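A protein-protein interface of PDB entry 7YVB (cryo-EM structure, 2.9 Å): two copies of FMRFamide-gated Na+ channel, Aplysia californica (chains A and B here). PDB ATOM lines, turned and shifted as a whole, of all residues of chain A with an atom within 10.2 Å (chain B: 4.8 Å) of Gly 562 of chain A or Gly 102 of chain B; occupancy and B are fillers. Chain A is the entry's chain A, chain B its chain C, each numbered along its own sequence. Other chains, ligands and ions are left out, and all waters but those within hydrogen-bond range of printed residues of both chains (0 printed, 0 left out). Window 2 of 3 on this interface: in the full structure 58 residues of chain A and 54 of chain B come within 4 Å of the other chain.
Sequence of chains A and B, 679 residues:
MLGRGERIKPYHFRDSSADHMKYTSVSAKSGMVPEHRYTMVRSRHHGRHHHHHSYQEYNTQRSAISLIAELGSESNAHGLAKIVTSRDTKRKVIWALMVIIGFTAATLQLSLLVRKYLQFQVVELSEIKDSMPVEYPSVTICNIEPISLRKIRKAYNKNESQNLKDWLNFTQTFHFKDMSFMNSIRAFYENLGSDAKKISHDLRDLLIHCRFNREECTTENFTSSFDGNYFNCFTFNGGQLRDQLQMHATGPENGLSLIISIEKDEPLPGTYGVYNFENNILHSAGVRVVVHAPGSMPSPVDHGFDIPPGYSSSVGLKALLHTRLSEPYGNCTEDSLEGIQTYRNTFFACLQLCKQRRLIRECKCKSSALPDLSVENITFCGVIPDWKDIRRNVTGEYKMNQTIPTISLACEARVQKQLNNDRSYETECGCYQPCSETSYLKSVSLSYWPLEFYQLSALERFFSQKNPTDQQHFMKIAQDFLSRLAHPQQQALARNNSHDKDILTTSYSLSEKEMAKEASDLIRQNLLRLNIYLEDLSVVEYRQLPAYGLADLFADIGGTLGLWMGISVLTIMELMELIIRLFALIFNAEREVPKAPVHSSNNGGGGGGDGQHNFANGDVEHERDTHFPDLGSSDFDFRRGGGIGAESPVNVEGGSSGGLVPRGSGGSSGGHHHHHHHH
The backbone carbonyl oxygen (O) of Gly 566 of chain A sits close to the side-chain sulfur (SD) of Met 98 of chain B (3.4 Å).
Among the printed residues, pairs that only touch across the chains: Gly 562 of chain A with Gly 102 of chain B (3.3 Å), Gly 562 of chain A with Ala 105 of chain B (3.8 Å), Leu 563 of chain A with Gly 102 of chain B (3.98 Å), Leu 563 of chain A with Trp 564 of chain B (3.7 Å) and Leu 570 of chain A with Met 98 of chain B (3.5 Å).
Leu 553 of chain A touches none of the printed residues of chain B. Of chain B, only Gly 102 (3.3 Å) and Ala 105 (3.8 Å) come within 4 Å of Gly 562 of chain A. Of the printed residues of chain B, Gly 566 of chain A touches Met 98 (3.4 Å). Printed residues of chain B within 4 Å of Leu 570 of chain A: Met 98 (3.5 Å). Gly 102 of chain B touches just these residues of chain A: Gly 562 (3.3 Å) and Leu 563 (3.98 Å). Phe 103 of chain B touches none of the printed residues of chain A. Ala 106 of chain B touches none of the printed residues of chain A. Printed residues of chain A within 4 Å of Trp 564 of chain B: Leu 563. The nearest residue of chain B that does not touch Gly 562 of chain A is Met 98 of chain B (4.4 Å). The nearest residue of chain A that does not touch Gly 102 of chain B is Gly 559 of chain A (5.4 Å).
Printed residues of chain B that touch a printed residue of chain A: Met 98, Gly 102, Ala 105 and Trp 564. Hydrophobic or aromatic side chains of chain B that line the printed part of chain A: Met 98, Ala 105 and Trp 564. Hydrophobic or aromatic side chains of chain A that line the printed part of chain B: Leu 563 and Leu 570. Among the printed residues, 6 pairs touch across the chains. Among the printed residues, no Asp or Glu carboxylate lies within 4 Å of a Lys or Arg side-chain nitrogen of the other chain.
Positions printed for both chains: 106 and 564. Of the 6 pairs that touch across the chains among the printed residues, none has its exchanged pair printed and touching as well.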
ATOM      1  N   ALA A 106     -27.255   2.036 -25.002  1.00  0.00           N
ATOM      2  CA  ALA A 106     -26.046   2.734 -24.581  1.00  0.00           C
ATOM      3  C   ALA A 106     -24.814   2.208 -25.304  1.00  0.00           C
ATOM      4  O   ALA A 106     -23.952   2.989 -25.721  1.00  0.00           O
ATOM      5  CB  ALA A 106     -25.872   2.615 -23.067  1.00  0.00           C
ATOM      6  N   LEU A 110     -22.299   4.111 -27.810  1.00  0.00           N
ATOM      7  CA  LEU A 110     -20.852   4.138 -27.622  1.00  0.00           C
ATOM      8  C   LEU A 110     -20.128   3.611 -28.854  1.00  0.00           C
ATOM      9  O   LEU A 110     -19.075   4.135 -29.237  1.00  0.00           O
ATOM     10  CB  LEU A 110     -20.472   3.330 -26.380  1.00  0.00           C
ATOM     11  CG  LEU A 110     -19.023   3.414 -25.899  1.00  0.00           C
ATOM     12  CD1 LEU A 110     -18.972   3.348 -24.384  1.00  0.00           C
ATOM     13  CD2 LEU A 110     -18.176   2.303 -26.499  1.00  0.00           C
ATOM     14  N   LEU A 553     -13.709  12.036 -27.480  1.00  0.00           N
ATOM     15  CA  LEU A 553     -14.235  10.687 -27.297  1.00  0.00           C
ATOM     16  C   LEU A 553     -14.336  10.338 -25.823  1.00  0.00           C
ATOM     17  O   LEU A 553     -15.356   9.811 -25.365  1.00  0.00           O
ATOM     18  CB  LEU A 553     -13.355   9.667 -28.023  1.00  0.00           C
ATOM     19  CG  LEU A 553     -13.821   8.207 -28.013  1.00  0.00           C
ATOM     20  CD1 LEU A 553     -13.385   7.500 -29.261  1.00  0.00           C
ATOM     21  CD2 LEU A 553     -13.274   7.460 -26.813  1.00  0.00           C
ATOM     22  N   PHE A 554     -13.267  10.600 -25.069  1.00  0.00           N
ATOM     23  CA  PHE A 554     -13.305  10.349 -23.633  1.00  0.00           C
ATOM     24  C   PHE A 554     -14.380  11.185 -22.945  1.00  0.00           C
ATOM     25  O   PHE A 554     -15.141  10.667 -22.119  1.00  0.00           O
ATOM     26  CB  PHE A 554     -11.922  10.582 -23.020  1.00  0.00           C
ATOM     27  CG  PHE A 554     -10.960   9.435 -23.245  1.00  0.00           C
ATOM     28  CD1 PHE A 554     -10.162   9.353 -24.379  1.00  0.00           C
ATOM     29  CD2 PHE A 554     -10.825   8.455 -22.278  1.00  0.00           C
ATOM     30  CE1 PHE A 554      -9.283   8.290 -24.549  1.00  0.00           C
ATOM     31  CE2 PHE A 554      -9.948   7.403 -22.446  1.00  0.00           C
ATOM     32  CZ  PHE A 554      -9.175   7.316 -23.580  1.00  0.00           C
ATOM     33  N   ALA A 555     -14.494  12.466 -23.306  1.00  0.00           N
ATOM     34  CA  ALA A 555     -15.513  13.319 -22.704  1.00  0.00           C
ATOM     35  C   ALA A 555     -16.922  12.846 -23.033  1.00  0.00           C
ATOM     36  O   ALA A 555     -17.858  13.125 -22.280  1.00  0.00           O
ATOM     37  CB  ALA A 555     -15.329  14.764 -23.167  1.00  0.00           C
ATOM     38  N   ASP A 556     -17.099  12.150 -24.154  1.00  0.00           N
ATOM     39  CA  ASP A 556     -18.424  11.715 -24.567  1.00  0.00           C
ATOM     40  C   ASP A 556     -18.745  10.275 -24.191  1.00  0.00           C
ATOM     41  O   ASP A 556     -19.913   9.883 -24.272  1.00  0.00           O
ATOM     42  CB  ASP A 556     -18.591  11.891 -26.079  1.00  0.00           C
ATOM     43  CG  ASP A 556     -18.959  13.308 -26.462  1.00  0.00           C
ATOM     44  OD1 ASP A 556     -19.824  13.903 -25.785  1.00  0.00           O
ATOM     45  OD2 ASP A 556     -18.383  13.830 -27.438  1.00  0.00           O
ATOM     46  N   ILE A 557     -17.756   9.474 -23.799  1.00  0.00           N
ATOM     47  CA  ILE A 557     -18.025   8.104 -23.403  1.00  0.00           C
ATOM     48  C   ILE A 557     -17.896   7.887 -21.899  1.00  0.00           C
ATOM     49  O   ILE A 557     -18.665   7.094 -21.343  1.00  0.00           O
ATOM     50  CB  ILE A 557     -17.147   7.091 -24.169  1.00  0.00           C
ATOM     51  CG1 ILE A 557     -15.692   7.162 -23.705  1.00  0.00           C
ATOM     52  CG2 ILE A 557     -17.268   7.300 -25.670  1.00  0.00           C
ATOM     53  CD1 ILE A 557     -14.887   5.929 -24.038  1.00  0.00           C
ATOM     54  N   GLY A 558     -16.979   8.583 -21.216  1.00  0.00           N
ATOM     55  CA  GLY A 558     -16.622   8.196 -19.859  1.00  0.00           C
ATOM     56  C   GLY A 558     -17.795   8.179 -18.897  1.00  0.00           C
ATOM     57  O   GLY A 558     -17.909   7.278 -18.063  1.00  0.00           O
ATOM     58  N   GLY A 559     -18.681   9.172 -18.997  1.00  0.00           N
ATOM     59  CA  GLY A 559     -19.812   9.232 -18.083  1.00  0.00           C
ATOM     60  C   GLY A 559     -20.696   8.004 -18.163  1.00  0.00           C
ATOM     61  O   GLY A 559     -21.110   7.454 -17.138  1.00  0.00           O
ATOM     62  N   THR A 560     -20.999   7.556 -19.381  1.00  0.00           N
ATOM     63  CA  THR A 560     -21.718   6.300 -19.560  1.00  0.00           C
ATOM     64  C   THR A 560     -20.871   5.118 -19.111  1.00  0.00           C
ATOM     65  O   THR A 560     -21.312   4.291 -18.304  1.00  0.00           O
ATOM     66  CB  THR A 560     -22.115   6.146 -21.028  1.00  0.00           C
ATOM     67  OG1 THR A 560     -23.051   7.170 -21.383  1.00  0.00           O
ATOM     68  CG2 THR A 560     -22.722   4.778 -21.284  1.00  0.00           C
ATOM     69  N   LEU A 561     -19.628   5.060 -19.590  1.00  0.00           N
ATOM     70  CA  LEU A 561     -18.813   3.858 -19.471  1.00  0.00           C
ATOM     71  C   LEU A 561     -18.530   3.514 -18.014  1.00  0.00           C
ATOM     72  O   LEU A 561     -18.539   2.335 -17.637  1.00  0.00           O
ATOM     73  CB  LEU A 561     -17.517   4.061 -20.257  1.00  0.00           C
ATOM     74  CG  LEU A 561     -16.533   2.923 -20.504  1.00  0.00           C
ATOM     75  CD1 LEU A 561     -15.941   3.101 -21.885  1.00  0.00           C
ATOM     76  CD2 LEU A 561     -15.442   2.949 -19.471  1.00  0.00           C
ATOM     77  N   GLY A 562     -18.297   4.531 -17.178  1.00  0.00           N
ATOM     78  CA  GLY A 562     -17.983   4.274 -15.780  1.00  0.00           C
ATOM     79  C   GLY A 562     -19.065   3.492 -15.059  1.00  0.00           C
ATOM     80  O   GLY A 562     -18.773   2.565 -14.301  1.00  0.00           O
ATOM     81  N   LEU A 563     -20.328   3.864 -15.274  1.00  0.00           N
ATOM     82  CA  LEU A 563     -21.441   3.132 -14.677  1.00  0.00           C
ATOM     83  C   LEU A 563     -21.744   1.838 -15.427  1.00  0.00           C
ATOM     84  O   LEU A 563     -22.115   0.831 -14.813  1.00  0.00           O
ATOM     85  CB  LEU A 563     -22.682   4.026 -14.629  1.00  0.00           C
ATOM     86  CG  LEU A 563     -23.949   3.450 -13.997  1.00  0.00           C
ATOM     87  CD1 LEU A 563     -23.732   3.152 -12.516  1.00  0.00           C
ATOM     88  CD2 LEU A 563     -25.124   4.386 -14.216  1.00  0.00           C
ATOM     89  N   TRP A 564     -21.594   1.832 -16.748  1.00  0.00           N
ATOM     90  CA  TRP A 564     -22.113   0.697 -17.509  1.00  0.00           C
ATOM     91  C   TRP A 564     -21.143  -0.484 -17.589  1.00  0.00           C
ATOM     92  O   TRP A 564     -21.601  -1.620 -17.746  1.00  0.00           O
ATOM     93  CB  TRP A 564     -22.566   1.154 -18.899  1.00  0.00           C
ATOM     94  CG  TRP A 564     -23.852   1.978 -18.806  1.00  0.00           C
ATOM     95  CD1 TRP A 564     -23.953   3.299 -18.487  1.00  0.00           C
ATOM     96  CD2 TRP A 564     -25.204   1.518 -19.000  1.00  0.00           C
ATOM     97  NE1 TRP A 564     -25.270   3.697 -18.482  1.00  0.00           N
ATOM     98  CE2 TRP A 564     -26.056   2.621 -18.795  1.00  0.00           C
ATOM     99  CE3 TRP A 564     -25.771   0.287 -19.334  1.00  0.00           C
ATOM    100  CZ2 TRP A 564     -27.438   2.531 -18.909  1.00  0.00           C
ATOM    101  CZ3 TRP A 564     -27.144   0.199 -19.443  1.00  0.00           C
ATOM    102  CH2 TRP A 564     -27.964   1.320 -19.236  1.00  0.00           C
ATOM    103  N   MET A 565     -19.832  -0.282 -17.413  1.00  0.00           N
ATOM    104  CA  MET A 565     -18.990  -1.446 -17.153  1.00  0.00           C
ATOM    105  C   MET A 565     -19.347  -2.107 -15.837  1.00  0.00           C
ATOM    106  O   MET A 565     -19.338  -3.344 -15.733  1.00  0.00           O
ATOM    107  CB  MET A 565     -17.513  -1.074 -17.155  1.00  0.00           C
ATOM    108  CG  MET A 565     -16.640  -2.102 -17.842  1.00  0.00           C
ATOM    109  SD  MET A 565     -14.904  -1.700 -17.870  1.00  0.00           S
ATOM    110  CE  MET A 565     -15.054   0.063 -17.713  1.00  0.00           C
ATOM    111  N   GLY A 566     -19.657  -1.297 -14.826  1.00  0.00           N
ATOM    112  CA  GLY A 566     -20.105  -1.852 -13.557  1.00  0.00           C
ATOM    113  C   GLY A 566     -21.405  -2.618 -13.686  1.00  0.00           C
ATOM    114  O   GLY A 566     -21.563  -3.700 -13.109  1.00  0.00           O
ATOM    115  N   ILE A 567     -22.348  -2.084 -14.467  1.00  0.00           N
ATOM    116  CA  ILE A 567     -23.603  -2.815 -14.648  1.00  0.00           C
ATOM    117  C   ILE A 567     -23.381  -4.062 -15.498  1.00  0.00           C
ATOM    118  O   ILE A 567     -24.092  -5.057 -15.340  1.00  0.00           O
ATOM    119  CB  ILE A 567     -24.704  -1.907 -15.236  1.00  0.00           C
ATOM    120  CG1 ILE A 567     -26.063  -2.590 -15.117  1.00  0.00           C
ATOM    121  CG2 ILE A 567     -24.477  -1.646 -16.691  1.00  0.00           C
ATOM    122  CD1 ILE A 567     -27.226  -1.667 -15.389  1.00  0.00           C
ATOM    123  N   SER A 568     -22.391  -4.048 -16.400  1.00  0.00           N
ATOM    124  CA  SER A 568     -22.032  -5.281 -17.100  1.00  0.00           C
ATOM    125  C   SER A 568     -21.498  -6.325 -16.127  1.00  0.00           C
ATOM    126  O   SER A 568     -21.803  -7.518 -16.253  1.00  0.00           O
ATOM    127  CB  SER A 568     -21.001  -4.998 -18.195  1.00  0.00           C
ATOM    128  OG  SER A 568     -19.681  -5.075 -17.685  1.00  0.00           O
ATOM    129  N   VAL A 569     -20.688  -5.895 -15.159  1.00  0.00           N
ATOM    130  CA  VAL A 569     -20.222  -6.816 -14.123  1.00  0.00           C
ATOM    131  C   VAL A 569     -21.407  -7.360 -13.329  1.00  0.00           C
ATOM    132  O   VAL A 569     -21.450  -8.547 -12.973  1.00  0.00           O
ATOM    133  CB  VAL A 569     -19.196  -6.120 -13.210  1.00  0.00           C
ATOM    134  CG1 VAL A 569     -18.816  -7.030 -12.054  1.00  0.00           C
ATOM    135  CG2 VAL A 569     -17.960  -5.724 -14.005  1.00  0.00           C
ATOM    136  N   LEU A 570     -22.385  -6.497 -13.040  1.00  0.00           N
ATOM    137  CA  LEU A 570     -23.615  -6.943 -12.388  1.00  0.00           C
ATOM    138  C   LEU A 570     -24.319  -8.012 -13.210  1.00  0.00           C
ATOM    139  O   LEU A 570     -24.793  -9.017 -12.665  1.00  0.00           O
ATOM    140  CB  LEU A 570     -24.564  -5.766 -12.169  1.00  0.00           C
ATOM    141  CG  LEU A 570     -24.451  -4.926 -10.904  1.00  0.00           C
ATOM    142  CD1 LEU A 570     -25.297  -3.674 -11.051  1.00  0.00           C
ATOM    143  CD2 LEU A 570     -24.882  -5.723  -9.684  1.00  0.00           C
ATOM    144  N   MET B  98     -17.635  -0.782  -7.747  1.00  0.00           N
ATOM    145  CA  MET B  98     -18.032  -0.385  -9.095  1.00  0.00           C
ATOM    146  C   MET B  98     -18.698   0.986  -9.087  1.00  0.00           C
ATOM    147  O   MET B  98     -18.505   1.779 -10.015  1.00  0.00           O
ATOM    148  CB  MET B  98     -18.953  -1.431  -9.721  1.00  0.00           C
ATOM    149  CG  MET B  98     -20.295  -1.581  -9.040  1.00  0.00           C
ATOM    150  SD  MET B  98     -21.324  -2.856  -9.780  1.00  0.00           S
ATOM    151  CE  MET B  98     -22.762  -2.739  -8.724  1.00  0.00           C
ATOM    152  N   VAL B  99     -19.467   1.294  -8.038  1.00  0.00           N
ATOM    153  CA  VAL B  99     -20.076   2.614  -7.935  1.00  0.00           C
ATOM    154  C   VAL B  99     -19.004   3.685  -7.789  1.00  0.00           C
ATOM    155  O   VAL B  99     -19.091   4.752  -8.401  1.00  0.00           O
ATOM    156  CB  VAL B  99     -21.084   2.647  -6.771  1.00  0.00           C
ATOM    157  CG1 VAL B  99     -21.336   4.076  -6.315  1.00  0.00           C
ATOM    158  CG2 VAL B  99     -22.390   1.980  -7.183  1.00  0.00           C
ATOM    159  N   ILE B 100     -17.975   3.417  -6.982  1.00  0.00           N
ATOM    160  CA  ILE B 100     -16.887   4.374  -6.808  1.00  0.00           C
ATOM    161  C   ILE B 100     -16.149   4.593  -8.122  1.00  0.00           C
ATOM    162  O   ILE B 100     -15.827   5.730  -8.489  1.00  0.00           O
ATOM    163  CB  ILE B 100     -15.935   3.899  -5.694  1.00  0.00           C
ATOM    164  CG1 ILE B 100     -16.535   4.191  -4.317  1.00  0.00           C
ATOM    165  CG2 ILE B 100     -14.567   4.552  -5.835  1.00  0.00           C
ATOM    166  CD1 ILE B 100     -15.798   3.520  -3.176  1.00  0.00           C
ATOM    167  N   ILE B 101     -15.868   3.510  -8.850  1.00  0.00           N
ATOM    168  CA  ILE B 101     -15.164   3.639 -10.125  1.00  0.00           C
ATOM    169  C   ILE B 101     -16.000   4.445 -11.114  1.00  0.00           C
ATOM    170  O   ILE B 101     -15.495   5.349 -11.793  1.00  0.00           O
ATOM    171  CB  ILE B 101     -14.806   2.250 -10.685  1.00  0.00           C
ATOM    172  CG1 ILE B 101     -13.669   1.631  -9.871  1.00  0.00           C
ATOM    173  CG2 ILE B 101     -14.425   2.344 -12.153  1.00  0.00           C
ATOM    174  CD1 ILE B 101     -13.162   0.317 -10.427  1.00  0.00           C
ATOM    175  N   GLY B 102     -17.296   4.135 -11.201  1.00  0.00           N
ATOM    176  CA  GLY B 102     -18.165   4.880 -12.095  1.00  0.00           C
ATOM    177  C   GLY B 102     -18.283   6.340 -11.713  1.00  0.00           C
ATOM    178  O   GLY B 102     -18.307   7.218 -12.579  1.00  0.00           O
ATOM    179  N   PHE B 103     -18.360   6.623 -10.412  1.00  0.00           N
ATOM    180  CA  PHE B 103     -18.434   8.004  -9.954  1.00  0.00           C
ATOM    181  C   PHE B 103     -17.168   8.766 -10.304  1.00  0.00           C
ATOM    182  O   PHE B 103     -17.233   9.907 -10.768  1.00  0.00           O
ATOM    183  CB  PHE B 103     -18.689   8.045  -8.447  1.00  0.00           C
ATOM    184  CG  PHE B 103     -18.577   9.418  -7.851  1.00  0.00           C
ATOM    185  CD1 PHE B 103     -19.652  10.287  -7.876  1.00  0.00           C
ATOM    186  CD2 PHE B 103     -17.397   9.838  -7.257  1.00  0.00           C
ATOM    187  CE1 PHE B 103     -19.554  11.551  -7.326  1.00  0.00           C
ATOM    188  CE2 PHE B 103     -17.291  11.100  -6.707  1.00  0.00           C
ATOM    189  CZ  PHE B 103     -18.373  11.957  -6.741  1.00  0.00           C
ATOM    190  N   THR B 104     -16.003   8.153 -10.079  1.00  0.00           N
ATOM    191  CA  THR B 104     -14.753   8.814 -10.429  1.00  0.00           C
ATOM    192  C   THR B 104     -14.675   9.075 -11.926  1.00  0.00           C
ATOM    193  O   THR B 104     -14.277  10.165 -12.350  1.00  0.00           O
ATOM    194  CB  THR B 104     -13.562   7.976  -9.966  1.00  0.00           C
ATOM    195  OG1 THR B 104     -13.729   6.621 -10.399  1.00  0.00           O
ATOM    196  CG2 THR B 104     -13.442   8.015  -8.450  1.00  0.00           C
ATOM    197  N   ALA B 105     -15.070   8.095 -12.741  1.00  0.00           N
ATOM    198  CA  ALA B 105     -15.052   8.287 -14.188  1.00  0.00           C
ATOM    199  C   ALA B 105     -15.983   9.422 -14.603  1.00  0.00           C
ATOM    200  O   ALA B 105     -15.596  10.310 -15.373  1.00  0.00           O
ATOM    201  CB  ALA B 105     -15.435   6.988 -14.894  1.00  0.00           C
ATOM    202  N   ALA B 106     -17.213   9.416 -14.086  1.00  0.00           N
ATOM    203  CA  ALA B 106     -18.188  10.429 -14.472  1.00  0.00           C
ATOM    204  C   ALA B 106     -17.760  11.820 -14.022  1.00  0.00           C
ATOM    205  O   ALA B 106     -17.902  12.791 -14.773  1.00  0.00           O
ATOM    206  CB  ALA B 106     -19.562  10.079 -13.901  1.00  0.00           C
ATOM    207  N   TRP B 564     -26.318  11.951 -10.788  1.00  0.00           N
ATOM    208  CA  TRP B 564     -25.117  11.692  -9.996  1.00  0.00           C
ATOM    209  C   TRP B 564     -24.978  12.601  -8.774  1.00  0.00           C
ATOM    210  O   TRP B 564     -24.337  12.195  -7.800  1.00  0.00           O
ATOM    211  CB  TRP B 564     -23.873  11.746 -10.889  1.00  0.00           C
ATOM    212  CG  TRP B 564     -23.813  10.525 -11.810  1.00  0.00           C
ATOM    213  CD1 TRP B 564     -24.483  10.356 -12.985  1.00  0.00           C
ATOM    214  CD2 TRP B 564     -23.070   9.307 -11.603  1.00  0.00           C
ATOM    215  NE1 TRP B 564     -24.200   9.125 -13.530  1.00  0.00           N
ATOM    216  CE2 TRP B 564     -23.335   8.464 -12.700  1.00  0.00           C
ATOM    217  CE3 TRP B 564     -22.207   8.855 -10.604  1.00  0.00           C
ATOM    218  CZ2 TRP B 564     -22.772   7.199 -12.826  1.00  0.00           C
ATOM    219  CZ3 TRP B 564     -21.652   7.598 -10.728  1.00  0.00           C
ATOM    220  CH2 TRP B 564     -21.934   6.785 -11.837  1.00  0.00           C
